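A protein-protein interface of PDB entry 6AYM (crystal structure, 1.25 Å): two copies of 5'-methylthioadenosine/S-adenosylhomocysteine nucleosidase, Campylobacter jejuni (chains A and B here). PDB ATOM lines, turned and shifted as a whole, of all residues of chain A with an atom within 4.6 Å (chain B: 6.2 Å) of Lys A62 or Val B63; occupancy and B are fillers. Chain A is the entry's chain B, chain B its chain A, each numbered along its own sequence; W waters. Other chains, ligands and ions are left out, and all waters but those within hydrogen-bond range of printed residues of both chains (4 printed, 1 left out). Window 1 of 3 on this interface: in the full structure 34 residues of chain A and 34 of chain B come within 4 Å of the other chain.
Among the printed residues, merely in contact across the chains: Lys A62 with Val B63, Val A63 with Lys B62, Val A63 with Thr B66, Val A63 with Gln B107, Val A63 with Ser B186, Thr A66 with Val B63, Thr A66 with Thr B66, Thr A66 with Leu B67, Gln A107 with Val B63, Gln A107 with Asp B159, Asp A159 with Gln B107, Asp A159 with Leu B110, Ser A186 with Val B63 and Leu A189 with Val B63.
Lys A62 touches Val B63, and with the chains exchanged Val A63 touches Lys B62.
Lys A62 touches Asp B159, and with the chains exchanged Asp A159 touches Lys B62.
Val A63 touches Gln B107, and with the chains exchanged Gln A107 touches Val B63.
Val A63 touches Ser B186, and with the chains exchanged Ser A186 touches Val B63.
Lys A62 touches just these residues of chain B: Val B63 and Asp B159.
Of the printed residues of chain A, Val B63 touches Lys A62 (3.9 Å), Thr A66 (3.5 Å), Gln A107 (3.6 Å), Ser A186 (3.7 Å) and Leu A189 (3.9 Å).
Of the printed residues of chain B, Leu A189 touches Val B63.
Of the printed residues of chain A, Asp B109 touches Asp A159 (3.3 Å).
Printed residues of chain B within 4 Å of Thr A66: Val B63, Thr B66 and Leu B67.
The nearest residue of chain B that does not touch Lys A62 is Lys B62 (4.3 Å).
The nearest printed residue of chain B that does not touch Gln A107 is Lys B62 (6.1 Å).
N of Lys B62 lies within hydrogen-bond range of OD1 of Asp B159, at 2.8 Å.
The backbone carbonyl oxygen (O) of Lys A62 is in hydrogen-bond range of the side-chain hydroxyl (OG1) of Thr A66, at 2.7 Å.
The backbone NH (N) of Asp B159 lies within hydrogen-bond range of the side-chain carboxylate (OD2) of Asp B109 (2.8 Å).
The side-chain carboxylate (OD1) of Asp B109 lies within salt-bridge range of the side-chain amino group (NZ) of Lys B62.
The side-chain hydroxyl (OG) of Ser B186 sits at hydrogen-bond distance from the side-chain hydroxyl (OG) of Ser B65 (2.9 Å).
NZ of Lys A62 is in salt-bridge range of OD1 of Asp A109 (2.7 Å).
Water W4 lies within hydrogen-bond range of the side-chain carboxylate of Asp A159 (2.6 Å), the side-chain amide oxygen of Gln B107 (2.8 Å), the backbone NH of Val A63 (2.9 Å) and the backbone NH of Lys A62 (3.3 Å).
Water W2 lies within hydrogen-bond range of OD2 of Asp B159 (2.6 Å), OE1 of Gln A107 (2.8 Å), N of Val B63 (2.9 Å) and N of Lys B62 (3.4 Å).
Water W3 bridges the side-chain carboxylate (OD2) of Asp B109 (2.7 Å) and the backbone carbonyl oxygen (O) of Asp A109 (2.8 Å).
Water W1 lies within hydrogen-bond range of the side-chain carboxylate (OD2) of Asp A109 (2.7 Å) and the backbone carbonyl oxygen (O) of Asp B109 (2.8 Å).
Of the 15 printed residues of chain B, 9 touch a printed residue of chain A.
Hydrophobic or aromatic side chains of chain B that line the printed part of chain A: Val B63 and Leu B110.
Hydrophobic or aromatic side chains of chain A within 4 Å of the printed part of chain B: Val A63 and Leu A189.
Along chain A the printed residues that touch a printed residue of chain B span positions 62 to 189.
Among the printed residues, 18 pairs touch across the chains.
Among the printed residues, Asp or Glu carboxylates within 4 Å of a Lys or Arg side-chain nitrogen of the other chain: Lys A62 with Asp B159 (2.8 Å) and Asp A159 with Lys B62 (2.7 Å).
O of Asp A159 sits close to O of Asp B109.
The side-chain amino group (NZ) of Lys B62 is in salt-bridge range of the side-chain carboxylate (OD2) of Asp A159 (2.7 Å).
The backbone carbonyl oxygen (O) of Asp A109 sits close to the backbone carbonyl oxygen (O) of Asp B159, at 3.3 Å.
NZ of Lys A62 is in salt-bridge range of OD2 of Asp B159, 2.8 Å away.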
ATOM      1  N   ILE A  60       8.798  -7.799  27.602  1.00  0.00           N
ATOM      2  CA  ILE A  60       7.384  -7.408  27.541  1.00  0.00           C
ATOM      3  C   ILE A  60       6.703  -7.951  26.288  1.00  0.00           C
ATOM      4  O   ILE A  60       7.191  -7.732  25.168  1.00  0.00           O
ATOM      5  CB  ILE A  60       7.223  -5.879  27.595  1.00  0.00           C
ATOM      6  CG1 ILE A  60       7.762  -5.346  28.924  1.00  0.00           C
ATOM      7  CG2 ILE A  60       5.767  -5.479  27.420  1.00  0.00           C
ATOM      8  CD1 ILE A  60       8.077  -3.862  28.911  1.00  0.00           C
ATOM      9  N   GLY A  61       5.556  -8.600  26.481  1.00  0.00           N
ATOM     10  CA  GLY A  61       4.676  -8.980  25.406  1.00  0.00           C
ATOM     11  C   GLY A  61       4.829 -10.406  24.924  1.00  0.00           C
ATOM     12  O   GLY A  61       5.677 -11.174  25.395  1.00  0.00           O
ATOM     13  N   LYS A  62       4.003 -10.754  23.941  1.00  0.00           N
ATOM     14  CA  LYS A  62       3.848 -12.144  23.506  1.00  0.00           C
ATOM     15  C   LYS A  62       5.111 -12.674  22.821  1.00  0.00           C
ATOM     16  O   LYS A  62       5.538 -13.807  23.094  1.00  0.00           O
ATOM     17  CB  LYS A  62       2.630 -12.311  22.589  1.00  0.00           C
ATOM     18  CG  LYS A  62       1.310 -12.082  23.299  1.00  0.00           C
ATOM     19  CD  LYS A  62       0.104 -12.580  22.496  1.00  0.00           C
ATOM     20  CE  LYS A  62       0.067 -11.981  21.097  1.00  0.00           C
ATOM     21  NZ  LYS A  62      -1.180 -12.362  20.380  1.00  0.00           N
ATOM     22  N   VAL A  63       5.662 -11.913  21.881  1.00  0.00           N
ATOM     23  CA  VAL A  63       6.858 -12.378  21.171  1.00  0.00           C
ATOM     24  C   VAL A  63       8.035 -12.553  22.140  1.00  0.00           C
ATOM     25  O   VAL A  63       8.722 -13.580  22.141  1.00  0.00           O
ATOM     26  CB  VAL A  63       7.223 -11.428  20.016  1.00  0.00           C
ATOM     27  CG1 VAL A  63       8.580 -11.767  19.428  1.00  0.00           C
ATOM     28  CG2 VAL A  63       6.136 -11.479  18.958  1.00  0.00           C
ATOM     29  N   ASN A  64       8.275 -11.535  22.958  1.00  0.00           N
ATOM     30  CA  ASN A  64       9.371 -11.613  23.911  1.00  0.00           C
ATOM     31  C   ASN A  64       9.245 -12.812  24.838  1.00  0.00           C
ATOM     32  O   ASN A  64      10.221 -13.534  25.075  1.00  0.00           O
ATOM     33  CB  ASN A  64       9.441 -10.340  24.771  1.00  0.00           C
ATOM     34  CG  ASN A  64      10.262  -9.247  24.143  1.00  0.00           C
ATOM     35  OD1 ASN A  64       9.863  -8.050  24.150  1.00  0.00           O
ATOM     36  ND2 ASN A  64      11.439  -9.608  23.697  1.00  0.00           N
ATOM     37  N   SER A  65       8.058 -13.014  25.397  1.00  0.00           N
ATOM     38  CA  SER A  65       7.861 -14.100  26.343  1.00  0.00           C
ATOM     39  C   SER A  65       7.910 -15.474  25.681  1.00  0.00           C
ATOM     40  O   SER A  65       8.445 -16.425  26.263  1.00  0.00           O
ATOM     41  CB  SER A  65       6.597 -13.882  27.155  1.00  0.00           C
ATOM     42  OG  SER A  65       5.436 -13.904  26.347  1.00  0.00           O
ATOM     43  N   THR A  66       7.411 -15.570  24.457  1.00  0.00           N
ATOM     44  CA  THR A  66       7.530 -16.808  23.688  1.00  0.00           C
ATOM     45  C   THR A  66       9.001 -17.156  23.492  1.00  0.00           C
ATOM     46  O   THR A  66       9.407 -18.308  23.704  1.00  0.00           O
ATOM     47  CB  THR A  66       6.859 -16.673  22.309  1.00  0.00           C
ATOM     48  OG1 THR A  66       5.460 -16.415  22.492  1.00  0.00           O
ATOM     49  CG2 THR A  66       7.021 -17.943  21.463  1.00  0.00           C
ATOM     50  N   GLN A 107      -5.415 -16.021  23.751  1.00  0.00           N
ATOM     51  CA  GLN A 107      -4.940 -14.774  23.166  1.00  0.00           C
ATOM     52  C   GLN A 107      -6.132 -13.992  22.626  1.00  0.00           C
ATOM     53  O   GLN A 107      -6.723 -14.370  21.596  1.00  0.00           O
ATOM     54  CB  GLN A 107      -3.946 -15.036  22.040  1.00  0.00           C
ATOM     55  CG  GLN A 107      -2.634 -15.643  22.531  1.00  0.00           C
ATOM     56  CD  GLN A 107      -1.769 -16.063  21.367  1.00  0.00           C
ATOM     57  OE1 GLN A 107      -1.319 -15.229  20.588  1.00  0.00           O
ATOM     58  NE2 GLN A 107      -1.569 -17.364  21.215  1.00  0.00           N
ATOM     59  N   ASP A 109      -6.243 -11.136  21.188  1.00  0.00           N
ATOM     60  CA  ASP A 109      -5.891 -10.350  20.003  1.00  0.00           C
ATOM     61  C   ASP A 109      -5.392 -11.190  18.831  1.00  0.00           C
ATOM     62  O   ASP A 109      -4.867 -10.646  17.851  1.00  0.00           O
ATOM     63  CB  ASP A 109      -4.888  -9.248  20.370  1.00  0.00           C
ATOM     64  CG  ASP A 109      -3.568  -9.777  20.891  1.00  0.00           C
ATOM     65  OD1 ASP A 109      -3.438 -11.001  21.137  1.00  0.00           O
ATOM     66  OD2 ASP A 109      -2.662  -8.926  21.062  1.00  0.00           O
ATOM     67  N   THR A 157      -4.650 -13.031  27.357  1.00  0.00           N
ATOM     68  CA  THR A 157      -3.347 -12.443  27.056  1.00  0.00           C
ATOM     69  C   THR A 157      -3.419 -11.723  25.716  1.00  0.00           C
ATOM     70  O   THR A 157      -4.056 -12.190  24.777  1.00  0.00           O
ATOM     71  CB  THR A 157      -2.269 -13.530  27.017  1.00  0.00           C
ATOM     72  OG1 THR A 157      -2.167 -14.141  28.308  1.00  0.00           O
ATOM     73  CG2 THR A 157      -0.924 -12.965  26.582  1.00  0.00           C
ATOM     74  N   GLY A 158      -2.784 -10.562  25.651  1.00  0.00           N
ATOM     75  CA  GLY A 158      -2.622  -9.878  24.395  1.00  0.00           C
ATOM     76  C   GLY A 158      -1.603  -8.778  24.530  1.00  0.00           C
ATOM     77  O   GLY A 158      -1.154  -8.465  25.608  1.00  0.00           O
ATOM     78  N   ASP A 159      -1.236  -8.203  23.393  1.00  0.00           N
ATOM     79  CA  ASP A 159      -0.119  -7.253  23.331  1.00  0.00           C
ATOM     80  C   ASP A 159      -0.508  -5.785  23.526  1.00  0.00           C
ATOM     81  O   ASP A 159       0.281  -4.894  23.243  1.00  0.00           O
ATOM     82  CB  ASP A 159       0.653  -7.456  22.023  1.00  0.00           C
ATOM     83  CG  ASP A 159       1.749  -8.489  22.154  1.00  0.00           C
ATOM     84  OD1 ASP A 159       2.185  -8.767  23.300  1.00  0.00           O
ATOM     85  OD2 ASP A 159       2.220  -8.970  21.096  1.00  0.00           O
ATOM     86  N   MET A 182       0.031  -9.621  29.351  1.00  0.00           N
ATOM     87  CA  MET A 182       0.678  -9.566  28.039  1.00  0.00           C
ATOM     88  C   MET A 182       1.610 -10.737  27.742  1.00  0.00           C
ATOM     89  O   MET A 182       2.211 -10.737  26.681  1.00  0.00           O
ATOM     90  CB  MET A 182       1.438  -8.243  27.919  1.00  0.00           C
ATOM     91  CG  MET A 182       0.554  -7.015  28.018  1.00  0.00           C
ATOM     92  SD  MET A 182       1.426  -5.440  27.948  1.00  0.00           S
ATOM     93  CE  MET A 182       1.977  -5.393  26.250  1.00  0.00           C
ATOM     94  N   SER A 186       1.080 -17.031  25.721  1.00  0.00           N
ATOM     95  CA  SER A 186       2.208 -17.346  24.852  1.00  0.00           C
ATOM     96  C   SER A 186       3.156 -18.327  25.522  1.00  0.00           C
ATOM     97  O   SER A 186       3.544 -19.336  24.926  1.00  0.00           O
ATOM     98  CB  SER A 186       2.916 -16.044  24.462  1.00  0.00           C
ATOM     99  OG  SER A 186       2.953 -15.112  25.522  1.00  0.00           O
ATOM    100  N   LEU A 189       1.517 -21.791  25.887  1.00  0.00           N
ATOM    101  CA  LEU A 189       1.521 -22.465  24.575  1.00  0.00           C
ATOM    102  C   LEU A 189       2.896 -23.088  24.271  1.00  0.00           C
ATOM    103  O   LEU A 189       2.974 -24.252  23.842  1.00  0.00           O
ATOM    104  CB  LEU A 189       1.109 -21.495  23.469  1.00  0.00           C
ATOM    105  CG  LEU A 189       1.123 -21.982  22.009  1.00  0.00           C
ATOM    106  CD1 LEU A 189       0.233 -21.117  21.147  1.00  0.00           C
ATOM    107  CD2 LEU A 189       2.544 -21.968  21.431  1.00  0.00           C
ATOM    108  N   ILE B  60       0.415 -20.120  12.263  1.00  0.00           N
ATOM    109  CA  ILE B  60      -0.176 -18.805  12.059  1.00  0.00           C
ATOM    110  C   ILE B  60       0.060 -17.881  13.242  1.00  0.00           C
ATOM    111  O   ILE B  60      -0.253 -18.242  14.392  1.00  0.00           O
ATOM    112  CB  ILE B  60      -1.688 -18.916  11.776  1.00  0.00           C
ATOM    113  CG1 ILE B  60      -1.913 -19.709  10.487  1.00  0.00           C
ATOM    114  CG2 ILE B  60      -2.328 -17.536  11.664  1.00  0.00           C
ATOM    115  CD1 ILE B  60      -3.314 -20.261  10.319  1.00  0.00           C
ATOM    116  N   GLY B  61       0.540 -16.673  12.944  1.00  0.00           N
ATOM    117  CA  GLY B  61       0.606 -15.599  13.898  1.00  0.00           C
ATOM    118  C   GLY B  61       1.942 -15.450  14.597  1.00  0.00           C
ATOM    119  O   GLY B  61       2.891 -16.224  14.394  1.00  0.00           O
ATOM    120  N   LYS B  62       1.995 -14.472  15.490  1.00  0.00           N
ATOM    121  CA  LYS B  62       3.261 -14.044  16.083  1.00  0.00           C
ATOM    122  C   LYS B  62       3.848 -15.090  17.025  1.00  0.00           C
ATOM    123  O   LYS B  62       5.063 -15.365  16.983  1.00  0.00           O
ATOM    124  CB  LYS B  62       3.100 -12.705  16.801  1.00  0.00           C
ATOM    125  CG  LYS B  62       2.802 -11.542  15.872  1.00  0.00           C
ATOM    126  CD  LYS B  62       2.957 -10.180  16.530  1.00  0.00           C
ATOM    127  CE  LYS B  62       2.169 -10.069  17.828  1.00  0.00           C
ATOM    128  NZ  LYS B  62       2.210  -8.704  18.400  1.00  0.00           N
ATOM    129  N   VAL B  63       3.041 -15.627  17.929  1.00  0.00           N
ATOM    130  CA  VAL B  63       3.540 -16.634  18.872  1.00  0.00           C
ATOM    131  C   VAL B  63       4.039 -17.883  18.140  1.00  0.00           C
ATOM    132  O   VAL B  63       5.134 -18.388  18.391  1.00  0.00           O
ATOM    133  CB  VAL B  63       2.490 -16.980  19.938  1.00  0.00           C
ATOM    134  CG1 VAL B  63       2.923 -18.178  20.766  1.00  0.00           C
ATOM    135  CG2 VAL B  63       2.229 -15.765  20.802  1.00  0.00           C
ATOM    136  N   ASN B  64       3.212 -18.395  17.242  1.00  0.00           N
ATOM    137  CA  ASN B  64       3.594 -19.584  16.485  1.00  0.00           C
ATOM    138  C   ASN B  64       4.888 -19.386  15.726  1.00  0.00           C
ATOM    139  O   ASN B  64       5.764 -20.255  15.745  1.00  0.00           O
ATOM    140  CB  ASN B  64       2.494 -19.980  15.499  1.00  0.00           C
ATOM    141  CG  ASN B  64       1.468 -20.904  16.114  1.00  0.00           C
ATOM    142  OD1 ASN B  64       1.837 -21.842  16.828  1.00  0.00           O
ATOM    143  ND2 ASN B  64       0.206 -20.702  15.805  1.00  0.00           N
ATOM    144  N   SER B  65       5.005 -18.261  15.031  1.00  0.00           N
ATOM    145  CA  SER B  65       6.186 -18.024  14.210  1.00  0.00           C
ATOM    146  C   SER B  65       7.431 -17.761  15.048  1.00  0.00           C
ATOM    147  O   SER B  65       8.520 -18.217  14.693  1.00  0.00           O
ATOM    148  CB  SER B  65       5.924 -16.924  13.190  1.00  0.00           C
ATOM    149  OG  SER B  65       5.663 -15.675  13.795  1.00  0.00           O
ATOM    150  N   THR B  66       7.266 -17.095  16.186  1.00  0.00           N
ATOM    151  CA  THR B  66       8.364 -16.909  17.117  1.00  0.00           C
ATOM    152  C   THR B  66       8.879 -18.258  17.595  1.00  0.00           C
ATOM    153  O   THR B  66      10.089 -18.501  17.607  1.00  0.00           O
ATOM    154  CB  THR B  66       7.908 -16.079  18.328  1.00  0.00           C
ATOM    155  OG1 THR B  66       7.507 -14.772  17.907  1.00  0.00           O
ATOM    156  CG2 THR B  66       9.017 -15.916  19.372  1.00  0.00           C
ATOM    157  N   LEU B  67       7.959 -19.135  17.994  1.00  0.00           N
ATOM    158  CA  LEU B  67       8.330 -20.465  18.453  1.00  0.00           C
ATOM    159  C   LEU B  67       9.045 -21.244  17.338  1.00  0.00           C
ATOM    160  O   LEU B  67      10.097 -21.817  17.567  1.00  0.00           O
ATOM    161  CB  LEU B  67       7.090 -21.231  18.947  1.00  0.00           C
ATOM    162  CG  LEU B  67       7.323 -22.677  19.377  1.00  0.00           C
ATOM    163  CD1 LEU B  67       8.386 -22.796  20.459  1.00  0.00           C
ATOM    164  CD2 LEU B  67       6.027 -23.312  19.833  1.00  0.00           C
ATOM    165  N   SER B  68       8.494 -21.250  16.138  1.00  0.00           N
ATOM    166  CA  SER B  68       9.111 -21.999  15.041  1.00  0.00           C
ATOM    167  C   SER B  68      10.528 -21.527  14.732  1.00  0.00           C
ATOM    168  O   SER B  68      11.433 -22.337  14.587  1.00  0.00           O
ATOM    169  CB  SER B  68       8.245 -21.925  13.791  1.00  0.00           C
ATOM    170  OG  SER B  68       6.984 -22.570  13.984  1.00  0.00           O
ATOM    171  N   GLN B 107       5.704  -4.374  14.908  1.00  0.00           N
ATOM    172  CA  GLN B 107       4.456  -4.987  15.373  1.00  0.00           C
ATOM    173  C   GLN B 107       3.425  -3.885  15.604  1.00  0.00           C
ATOM    174  O   GLN B 107       3.530  -3.119  16.568  1.00  0.00           O
ATOM    175  CB  GLN B 107       4.681  -5.771  16.661  1.00  0.00           C
ATOM    176  CG  GLN B 107       5.568  -7.000  16.494  1.00  0.00           C
ATOM    177  CD  GLN B 107       5.883  -7.617  17.822  1.00  0.00           C
ATOM    178  OE1 GLN B 107       5.021  -8.092  18.547  1.00  0.00           O
ATOM    179  NE2 GLN B 107       7.153  -7.590  18.173  1.00  0.00           N
ATOM    180  N   ASP B 109       0.379  -4.074  16.599  1.00  0.00           N
ATOM    181  CA  ASP B 109      -0.522  -4.384  17.715  1.00  0.00           C
ATOM    182  C   ASP B 109       0.181  -4.563  19.055  1.00  0.00           C
ATOM    183  O   ASP B 109      -0.425  -5.036  20.020  1.00  0.00           O
ATOM    184  CB  ASP B 109      -1.378  -5.596  17.361  1.00  0.00           C
ATOM    185  CG  ASP B 109      -0.572  -6.871  17.140  1.00  0.00           C
ATOM    186  OD1 ASP B 109       0.698  -6.820  17.103  1.00  0.00           O
ATOM    187  OD2 ASP B 109      -1.240  -7.929  17.012  1.00  0.00           O
ATOM    188  N   LEU B 110       1.451  -4.155  19.132  1.00  0.00           N
ATOM    189  CA  LEU B 110       2.194  -4.112  20.390  1.00  0.00           C
ATOM    190  C   LEU B 110       2.056  -2.695  20.922  1.00  0.00           C
ATOM    191  O   LEU B 110       2.622  -1.763  20.352  1.00  0.00           O
ATOM    192  CB  LEU B 110       3.652  -4.526  20.164  1.00  0.00           C
ATOM    193  CG  LEU B 110       4.551  -4.603  21.391  1.00  0.00           C
ATOM    194  CD1 LEU B 110       3.989  -5.516  22.469  1.00  0.00           C
ATOM    195  CD2 LEU B 110       5.962  -5.041  21.004  1.00  0.00           C
ATOM    196  N   ASP B 159      -1.356  -9.729  14.828  1.00  0.00           N
ATOM    197  CA  ASP B 159      -2.115 -10.972  14.943  1.00  0.00           C
ATOM    198  C   ASP B 159      -3.572 -10.871  14.501  1.00  0.00           C
ATOM    199  O   ASP B 159      -4.369 -11.774  14.795  1.00  0.00           O
ATOM    200  CB  ASP B 159      -2.011 -11.517  16.371  1.00  0.00           C
ATOM    201  CG  ASP B 159      -0.826 -12.426  16.575  1.00  0.00           C
ATOM    202  OD1 ASP B 159      -0.307 -12.945  15.557  1.00  0.00           O
ATOM    203  OD2 ASP B 159      -0.456 -12.671  17.744  1.00  0.00           O
ATOM    204  N   MET B 182       1.218 -11.493   9.348  1.00  0.00           N
ATOM    205  CA  MET B 182       1.037 -11.960  10.720  1.00  0.00           C
ATOM    206  C   MET B 182       2.263 -12.631  11.347  1.00  0.00           C
ATOM    207  O   MET B 182       2.180 -13.072  12.496  1.00  0.00           O
ATOM    208  CB  MET B 182      -0.165 -12.913  10.785  1.00  0.00           C
ATOM    209  CG  MET B 182      -1.466 -12.282  10.334  1.00  0.00           C
ATOM    210  SD  MET B 182      -2.880 -13.404  10.382  1.00  0.00           S
ATOM    211  CE  MET B 182      -3.153 -13.678  12.122  1.00  0.00           C
ATOM    212  N   SER B 186       7.988 -10.819  14.136  1.00  0.00           N
ATOM    213  CA  SER B 186       8.310 -11.753  15.204  1.00  0.00           C
ATOM    214  C   SER B 186       9.513 -12.614  14.832  1.00  0.00           C
ATOM    215  O   SER B 186      10.451 -12.745  15.610  1.00  0.00           O
ATOM    216  CB  SER B 186       7.083 -12.614  15.520  1.00  0.00           C
ATOM    217  OG  SER B 186       6.342 -12.931  14.356  1.00  0.00           O
HETATM  218  O   HOH W   1      -2.867  -6.220  20.620  1.00  0.00           O
HETATM  219  O   HOH W   2       0.154 -15.176  18.219  1.00  0.00           O
HETATM  220  O   HOH W   3      -3.976  -8.125  17.030  1.00  0.00           O
HETATM  221  O   HOH W   4       4.803  -9.211  21.109  1.00  0.00           O
